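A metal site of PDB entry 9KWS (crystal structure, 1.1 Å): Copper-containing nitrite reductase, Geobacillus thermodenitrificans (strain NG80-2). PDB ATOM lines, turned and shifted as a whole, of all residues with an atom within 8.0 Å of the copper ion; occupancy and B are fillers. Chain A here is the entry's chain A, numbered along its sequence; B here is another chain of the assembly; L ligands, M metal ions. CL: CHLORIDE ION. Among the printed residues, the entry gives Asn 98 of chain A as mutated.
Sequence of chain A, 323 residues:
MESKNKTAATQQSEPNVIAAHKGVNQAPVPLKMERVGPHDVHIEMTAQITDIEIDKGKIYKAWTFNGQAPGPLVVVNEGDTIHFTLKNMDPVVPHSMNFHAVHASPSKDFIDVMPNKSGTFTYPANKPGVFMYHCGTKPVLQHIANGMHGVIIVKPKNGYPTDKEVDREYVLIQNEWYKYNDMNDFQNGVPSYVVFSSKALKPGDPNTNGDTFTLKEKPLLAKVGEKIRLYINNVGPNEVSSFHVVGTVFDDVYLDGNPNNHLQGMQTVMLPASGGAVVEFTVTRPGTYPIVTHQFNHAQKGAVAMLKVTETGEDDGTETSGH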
ATOM      1  N   ASN A  98       0.530  29.000 -16.663  1.00  0.00           N
ATOM      2  CA  ASN A  98       1.594  28.009 -16.873  1.00  0.00           C
ATOM      3  C   ASN A  98       1.660  27.808 -18.389  1.00  0.00           C
ATOM      4  O   ASN A  98       0.702  27.349 -18.996  1.00  0.00           O
ATOM      5  CB  ASN A  98       1.153  26.717 -16.182  1.00  0.00           C
ATOM      6  CG  ASN A  98       2.073  25.547 -16.417  1.00  0.00           C
ATOM      7  OD1 ASN A  98       2.747  25.453 -17.429  1.00  0.00           O
ATOM      8  ND2 ASN A  98       2.007  24.577 -15.513  1.00  0.00           N
ATOM      9  N   PHE A  99       2.785  28.186 -19.001  1.00  0.00           N
ATOM     10  CA  PHE A  99       3.047  27.854 -20.399  1.00  0.00           C
ATOM     11  C   PHE A  99       3.949  26.633 -20.448  1.00  0.00           C
ATOM     12  O   PHE A  99       5.075  26.672 -19.934  1.00  0.00           O
ATOM     13  CB  PHE A  99       3.796  28.988 -21.117  1.00  0.00           C
ATOM     14  CG  PHE A  99       2.990  30.247 -21.393  1.00  0.00           C
ATOM     15  CD1 PHE A  99       2.075  30.300 -22.431  1.00  0.00           C
ATOM     16  CD2 PHE A  99       3.219  31.394 -20.654  1.00  0.00           C
ATOM     17  CE1 PHE A  99       1.378  31.462 -22.700  1.00  0.00           C
ATOM     18  CE2 PHE A  99       2.521  32.556 -20.923  1.00  0.00           C
ATOM     19  CZ  PHE A  99       1.607  32.594 -21.945  1.00  0.00           C
ATOM     20  N   HIS A 100       3.519  25.558 -21.117  1.00  0.00           N
ATOM     21  CA  HIS A 100       4.406  24.399 -21.254  1.00  0.00           C
ATOM     22  C   HIS A 100       5.620  24.696 -22.125  1.00  0.00           C
ATOM     23  O   HIS A 100       6.595  23.938 -22.092  1.00  0.00           O
ATOM     24  CB  HIS A 100       3.658  23.207 -21.839  1.00  0.00           C
ATOM     25  CG  HIS A 100       2.752  22.524 -20.880  1.00  0.00           C
ATOM     26  ND1 HIS A 100       2.265  21.257 -21.132  1.00  0.00           N
ATOM     27  CD2 HIS A 100       2.258  22.877 -19.667  1.00  0.00           C
ATOM     28  CE1 HIS A 100       1.511  20.873 -20.121  1.00  0.00           C
ATOM     29  NE2 HIS A 100       1.487  21.828 -19.209  1.00  0.00           N
ATOM     30  N   PHE A 110       4.832  31.154 -12.092  1.00  0.00           N
ATOM     31  CA  PHE A 110       3.488  30.687 -12.410  1.00  0.00           C
ATOM     32  C   PHE A 110       2.545  30.921 -11.221  1.00  0.00           C
ATOM     33  O   PHE A 110       1.609  30.167 -10.993  1.00  0.00           O
ATOM     34  CB  PHE A 110       3.474  29.198 -12.793  1.00  0.00           C
ATOM     35  CG  PHE A 110       4.256  28.800 -14.030  1.00  0.00           C
ATOM     36  CD1 PHE A 110       4.730  29.695 -14.979  1.00  0.00           C
ATOM     37  CD2 PHE A 110       4.458  27.442 -14.268  1.00  0.00           C
ATOM     38  CE1 PHE A 110       5.404  29.256 -16.113  1.00  0.00           C
ATOM     39  CE2 PHE A 110       5.111  26.995 -15.397  1.00  0.00           C
ATOM     40  CZ  PHE A 110       5.584  27.902 -16.328  1.00  0.00           C
ATOM     41  N   MET A 132       0.752  23.160 -24.664  1.00  0.00           N
ATOM     42  CA  MET A 132      -0.376  23.611 -23.874  1.00  0.00           C
ATOM     43  C   MET A 132       0.019  24.796 -23.005  1.00  0.00           C
ATOM     44  O   MET A 132       1.140  24.873 -22.512  1.00  0.00           O
ATOM     45  CB  MET A 132      -0.892  22.460 -23.022  1.00  0.00           C
ATOM     46  CG  MET A 132      -2.073  22.810 -22.144  1.00  0.00           C
ATOM     47  SD  MET A 132      -2.728  21.326 -21.365  1.00  0.00           S
ATOM     48  CE  MET A 132      -4.058  22.024 -20.376  1.00  0.00           C
ATOM     49  N   TYR A 133      -0.944  25.674 -22.766  1.00  0.00           N
ATOM     50  CA  TYR A 133      -0.893  26.601 -21.651  1.00  0.00           C
ATOM     51  C   TYR A 133      -2.174  26.449 -20.846  1.00  0.00           C
ATOM     52  O   TYR A 133      -3.197  26.002 -21.367  1.00  0.00           O
ATOM     53  CB  TYR A 133      -0.625  28.058 -22.091  1.00  0.00           C
ATOM     54  CG  TYR A 133      -1.744  28.800 -22.784  1.00  0.00           C
ATOM     55  CD1 TYR A 133      -2.873  29.223 -22.090  1.00  0.00           C
ATOM     56  CD2 TYR A 133      -1.637  29.167 -24.125  1.00  0.00           C
ATOM     57  CE1 TYR A 133      -3.860  29.971 -22.708  1.00  0.00           C
ATOM     58  CE2 TYR A 133      -2.612  29.924 -24.760  1.00  0.00           C
ATOM     59  CZ  TYR A 133      -3.727  30.310 -24.033  1.00  0.00           C
ATOM     60  OH  TYR A 133      -4.741  31.066 -24.600  1.00  0.00           O
ATOM     61  N   HIS A 134      -2.136  26.852 -19.583  1.00  0.00           N
ATOM     62  CA  HIS A 134      -3.317  26.738 -18.749  1.00  0.00           C
ATOM     63  C   HIS A 134      -3.107  27.492 -17.452  1.00  0.00           C
ATOM     64  O   HIS A 134      -1.993  27.781 -17.051  1.00  0.00           O
ATOM     65  CB  HIS A 134      -3.653  25.261 -18.452  1.00  0.00           C
ATOM     66  CG  HIS A 134      -2.545  24.513 -17.777  1.00  0.00           C
ATOM     67  ND1 HIS A 134      -2.386  24.479 -16.407  1.00  0.00           N
ATOM     68  CD2 HIS A 134      -1.547  23.736 -18.279  1.00  0.00           C
ATOM     69  CE1 HIS A 134      -1.350  23.708 -16.101  1.00  0.00           C
ATOM     70  NE2 HIS A 134      -0.820  23.256 -17.217  1.00  0.00           N
ATOM     71  N   CYS A 135      -4.209  27.753 -16.758  1.00  0.00           N
ATOM     72  CA  CYS A 135      -4.104  28.279 -15.413  1.00  0.00           C
ATOM     73  C   CYS A 135      -3.493  27.225 -14.495  1.00  0.00           C
ATOM     74  O   CYS A 135      -3.787  26.032 -14.608  1.00  0.00           O
ATOM     75  CB  CYS A 135      -5.482  28.675 -14.920  1.00  0.00           C
ATOM     76  SG  CYS A 135      -5.491  29.355 -13.236  1.00  0.00           S
ATOM     77  N   GLY A 136      -2.630  27.678 -13.596  1.00  0.00           N
ATOM     78  CA  GLY A 136      -1.941  26.817 -12.660  1.00  0.00           C
ATOM     79  C   GLY A 136      -2.339  26.999 -11.214  1.00  0.00           C
ATOM     80  O   GLY A 136      -1.565  26.655 -10.320  1.00  0.00           O
ATOM     81  N   VAL A 140      -5.659  22.697  -9.718  1.00  0.00           N
ATOM     82  CA  VAL A 140      -5.450  22.926 -11.142  1.00  0.00           C
ATOM     83  C   VAL A 140      -6.512  22.233 -11.974  1.00  0.00           C
ATOM     84  O   VAL A 140      -6.982  22.787 -12.963  1.00  0.00           O
ATOM     85  CB  VAL A 140      -4.014  22.517 -11.530  1.00  0.00           C
ATOM     86  CG1 VAL A 140      -3.815  22.595 -13.024  1.00  0.00           C
ATOM     87  CG2 VAL A 140      -3.008  23.394 -10.812  1.00  0.00           C
ATOM     88  N   ILE A 144      -8.459  24.153 -15.030  1.00  0.00           N
ATOM     89  CA  ILE A 144      -8.441  23.648 -16.404  1.00  0.00           C
ATOM     90  C   ILE A 144      -9.844  23.236 -16.824  1.00  0.00           C
ATOM     91  O   ILE A 144     -10.331  23.626 -17.897  1.00  0.00           O
ATOM     92  CB  ILE A 144      -7.439  22.495 -16.566  1.00  0.00           C
ATOM     93  CG1 ILE A 144      -6.004  22.938 -16.258  1.00  0.00           C
ATOM     94  CG2 ILE A 144      -7.549  21.947 -17.994  1.00  0.00           C
ATOM     95  CD1 ILE A 144      -4.994  21.814 -16.330  1.00  0.00           C
ATOM     96  N   VAL A 235      -5.763  19.310 -24.830  1.00  0.00           N
ATOM     97  CA  VAL A 235      -5.545  19.928 -23.521  1.00  0.00           C
ATOM     98  C   VAL A 235      -6.235  19.195 -22.386  1.00  0.00           C
ATOM     99  O   VAL A 235      -6.020  19.540 -21.209  1.00  0.00           O
ATOM    100  CB  VAL A 235      -5.907  21.428 -23.525  1.00  0.00           C
ATOM    101  CG1 VAL A 235      -5.050  22.185 -24.532  1.00  0.00           C
ATOM    102  CG2 VAL A 235      -7.385  21.654 -23.773  1.00  0.00           C
ATOM    103  N   ALA A 273      -2.744  13.634 -22.448  1.00  0.00           N
ATOM    104  CA  ALA A 273      -3.302  14.890 -21.980  1.00  0.00           C
ATOM    105  C   ALA A 273      -2.171  15.911 -21.930  1.00  0.00           C
ATOM    106  O   ALA A 273      -1.125  15.635 -21.323  1.00  0.00           O
ATOM    107  CB  ALA A 273      -3.940  14.714 -20.600  1.00  0.00           C
ATOM    108  N   SER A 274      -2.394  17.056 -22.574  1.00  0.00           N
ATOM    109  CA  SER A 274      -1.445  18.148 -22.866  1.00  0.00           C
ATOM    110  C   SER A 274      -0.574  17.871 -24.078  1.00  0.00           C
ATOM    111  O   SER A 274       0.261  18.723 -24.429  1.00  0.00           O
ATOM    112  CB  SER A 274      -0.576  18.593 -21.684  1.00  0.00           C
ATOM    113  OG  SER A 274       0.472  17.697 -21.394  1.00  0.00           O
ATOM    114  N   HIS B 244       4.617  14.758 -17.024  1.00  0.00           N
ATOM    115  CA  HIS B 244       5.029  16.136 -17.293  1.00  0.00           C
ATOM    116  C   HIS B 244       5.696  16.741 -16.069  1.00  0.00           C
ATOM    117  O   HIS B 244       5.205  16.577 -14.956  1.00  0.00           O
ATOM    118  CB  HIS B 244       3.764  16.958 -17.630  1.00  0.00           C
ATOM    119  CG  HIS B 244       4.012  18.417 -17.845  1.00  0.00           C
ATOM    120  ND1 HIS B 244       4.615  18.913 -18.979  1.00  0.00           N
ATOM    121  CD2 HIS B 244       3.759  19.502 -17.062  1.00  0.00           C
ATOM    122  CE1 HIS B 244       4.706  20.223 -18.903  1.00  0.00           C
ATOM    123  NE2 HIS B 244       4.197  20.609 -17.746  1.00  0.00           N
ATOM    124  N   VAL B 245       6.788  17.485 -16.298  1.00  0.00           N
ATOM    125  CA  VAL B 245       7.426  18.281 -15.256  1.00  0.00           C
ATOM    126  C   VAL B 245       7.120  19.755 -15.528  1.00  0.00           C
ATOM    127  O   VAL B 245       7.426  20.278 -16.600  1.00  0.00           O
ATOM    128  CB  VAL B 245       8.935  18.012 -15.150  1.00  0.00           C
ATOM    129  CG1 VAL B 245       9.553  18.888 -14.056  1.00  0.00           C
ATOM    130  CG2 VAL B 245       9.212  16.543 -14.868  1.00  0.00           C
ATOM    131  N   VAL B 246       6.498  20.400 -14.544  1.00  0.00           N
ATOM    132  CA  VAL B 246       6.123  21.803 -14.672  1.00  0.00           C
ATOM    133  C   VAL B 246       7.356  22.685 -14.706  1.00  0.00           C
ATOM    134  O   VAL B 246       8.287  22.504 -13.915  1.00  0.00           O
ATOM    135  CB  VAL B 246       5.217  22.180 -13.482  1.00  0.00           C
ATOM    136  CG1 VAL B 246       4.798  23.634 -13.561  1.00  0.00           C
ATOM    137  CG2 VAL B 246       3.989  21.290 -13.443  1.00  0.00           C
ATOM    138  N   GLY B 247       7.376  23.674 -15.604  1.00  0.00           N
ATOM    139  CA  GLY B 247       8.446  24.644 -15.653  1.00  0.00           C
ATOM    140  C   GLY B 247       9.639  24.255 -16.482  1.00  0.00           C
ATOM    141  O   GLY B 247      10.651  24.979 -16.490  1.00  0.00           O
ATOM    142  N   GLN B 267       7.042  18.012 -24.280  1.00  0.00           N
ATOM    143  CA  GLN B 267       6.432  18.583 -23.087  1.00  0.00           C
ATOM    144  C   GLN B 267       5.951  17.509 -22.118  1.00  0.00           C
ATOM    145  O   GLN B 267       6.051  17.683 -20.901  1.00  0.00           O
ATOM    146  CB  GLN B 267       5.283  19.532 -23.451  1.00  0.00           C
ATOM    147  CG  GLN B 267       3.987  18.904 -23.955  1.00  0.00           C
ATOM    148  CD  GLN B 267       3.114  19.941 -24.598  1.00  0.00           C
ATOM    149  OE1 GLN B 267       2.646  20.880 -23.945  1.00  0.00           O
ATOM    150  NE2 GLN B 267       2.922  19.805 -25.896  1.00  0.00           N
ATOM    151  N   THR B 268       5.440  16.399 -22.660  1.00  0.00           N
ATOM    152  CA  THR B 268       4.710  15.391 -21.913  1.00  0.00           C
ATOM    153  C   THR B 268       4.979  14.049 -22.577  1.00  0.00           C
ATOM    154  O   THR B 268       4.971  13.956 -23.808  1.00  0.00           O
ATOM    155  CB  THR B 268       3.224  15.730 -21.903  1.00  0.00           C
ATOM    156  OG1 THR B 268       3.100  16.968 -21.197  1.00  0.00           O
ATOM    157  CG2 THR B 268       2.377  14.640 -21.237  1.00  0.00           C
ATOM    158  N   VAL B 292       3.839  15.794 -12.519  1.00  0.00           N
ATOM    159  CA  VAL B 292       2.458  15.341 -12.582  1.00  0.00           C
ATOM    160  C   VAL B 292       2.270  14.262 -13.632  1.00  0.00           C
ATOM    161  O   VAL B 292       3.054  14.131 -14.575  1.00  0.00           O
ATOM    162  CB  VAL B 292       1.483  16.509 -12.870  1.00  0.00           C
ATOM    163  CG1 VAL B 292       1.712  17.652 -11.894  1.00  0.00           C
ATOM    164  CG2 VAL B 292       1.622  17.027 -14.307  1.00  0.00           C
ATOM    165  N   THR B 293       1.161  13.518 -13.502  1.00  0.00           N
ATOM    166  CA  THR B 293       0.472  13.051 -14.686  1.00  0.00           C
ATOM    167  C   THR B 293      -0.526  14.149 -15.074  1.00  0.00           C
ATOM    168  O   THR B 293      -1.258  14.665 -14.220  1.00  0.00           O
ATOM    169  CB  THR B 293      -0.219  11.695 -14.530  1.00  0.00           C
ATOM    170  OG1 THR B 293      -0.917  11.450 -15.754  1.00  0.00           O
ATOM    171  CG2 THR B 293      -1.169  11.659 -13.351  1.00  0.00           C
ATOM    172  N   HIS B 294      -0.519  14.522 -16.347  1.00  0.00           N
ATOM    173  CA  HIS B 294      -1.331  15.625 -16.816  1.00  0.00           C
ATOM    174  C   HIS B 294      -2.777  15.235 -17.078  1.00  0.00           C
ATOM    175  O   HIS B 294      -3.565  16.081 -17.509  1.00  0.00           O
ATOM    176  CB  HIS B 294      -0.704  16.286 -18.057  1.00  0.00           C
ATOM    177  CG  HIS B 294      -0.817  17.773 -18.049  1.00  0.00           C
ATOM    178  ND1 HIS B 294      -1.969  18.458 -18.325  1.00  0.00           N
ATOM    179  CD2 HIS B 294       0.103  18.722 -17.728  1.00  0.00           C
ATOM    180  CE1 HIS B 294      -1.753  19.761 -18.188  1.00  0.00           C
ATOM    181  NE2 HIS B 294      -0.496  19.944 -17.820  1.00  0.00           N
ATOM    182  N   PHE B 296      -5.539  15.245 -15.292  1.00  0.00           N
ATOM    183  CA  PHE B 296      -5.589  16.008 -14.043  1.00  0.00           C
ATOM    184  C   PHE B 296      -6.550  15.432 -13.025  1.00  0.00           C
ATOM    185  O   PHE B 296      -6.429  15.751 -11.830  1.00  0.00           O
ATOM    186  CB  PHE B 296      -5.747  17.520 -14.284  1.00  0.00           C
ATOM    187  CG  PHE B 296      -4.466  18.246 -14.027  1.00  0.00           C
ATOM    188  CD1 PHE B 296      -4.117  18.600 -12.735  1.00  0.00           C
ATOM    189  CD2 PHE B 296      -3.548  18.473 -15.046  1.00  0.00           C
ATOM    190  CE1 PHE B 296      -2.872  19.169 -12.482  1.00  0.00           C
ATOM    191  CE2 PHE B 296      -2.316  19.048 -14.792  1.00  0.00           C
ATOM    192  CZ  PHE B 296      -1.973  19.389 -13.513  1.00  0.00           C
HETATM  193 CL    CL L   1       1.187  21.253 -15.394  1.00  0.00          CL
HETATM  194 CU    CU M   1       0.424  21.720 -17.536  1.00  0.00          CU
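A ring nitrogen (ND1) of His 244 of chain B sits at hydrogen-bond distance from the backbone carbonyl oxygen (O) of Gln 267 of chain B (2.7 Å). A ring nitrogen (ND1) of His 100 sits at hydrogen-bond distance from the side-chain amide oxygen (OE1) of Gln 267 of chain B (2.9 Å). The backbone carbonyl oxygen (O) of His 244 of chain B is in hydrogen-bond range of the backbone NH (N) of Val 292 of chain B (2.9 Å). A ring nitrogen (NE2) of His 244 of chain B lies close to a ring nitrogen (NE2) of His 100 (3.3 Å). N of Asn 98 is in hydrogen-bond range of O of His 134. O of Met 132 is in hydrogen-bond range of N of His 100, at 2.8 Å. OG1 of Thr 268 of chain B is in hydrogen-bond range of ND1 of His 244 of chain B (3.3 Å).
Asn 98 touches the copper ion. NE2 of His 244 of chain B touches the copper ion (3.9 Å). Five residues have an atom within 4 Å of the copper ion: Asn 98, His 100, His 134, His 244 of chain B and His 294 of chain B.
NE2 of His 100 binds the copper ion (2.0 Å). NE2 of His 134 binds the copper ion, 2.0 Å away. NE2 of His 294 of chain B is bound to the copper ion. CL of the ligand binds the copper ion (2.3 Å). The copper ion has four donor atoms within binding distance.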
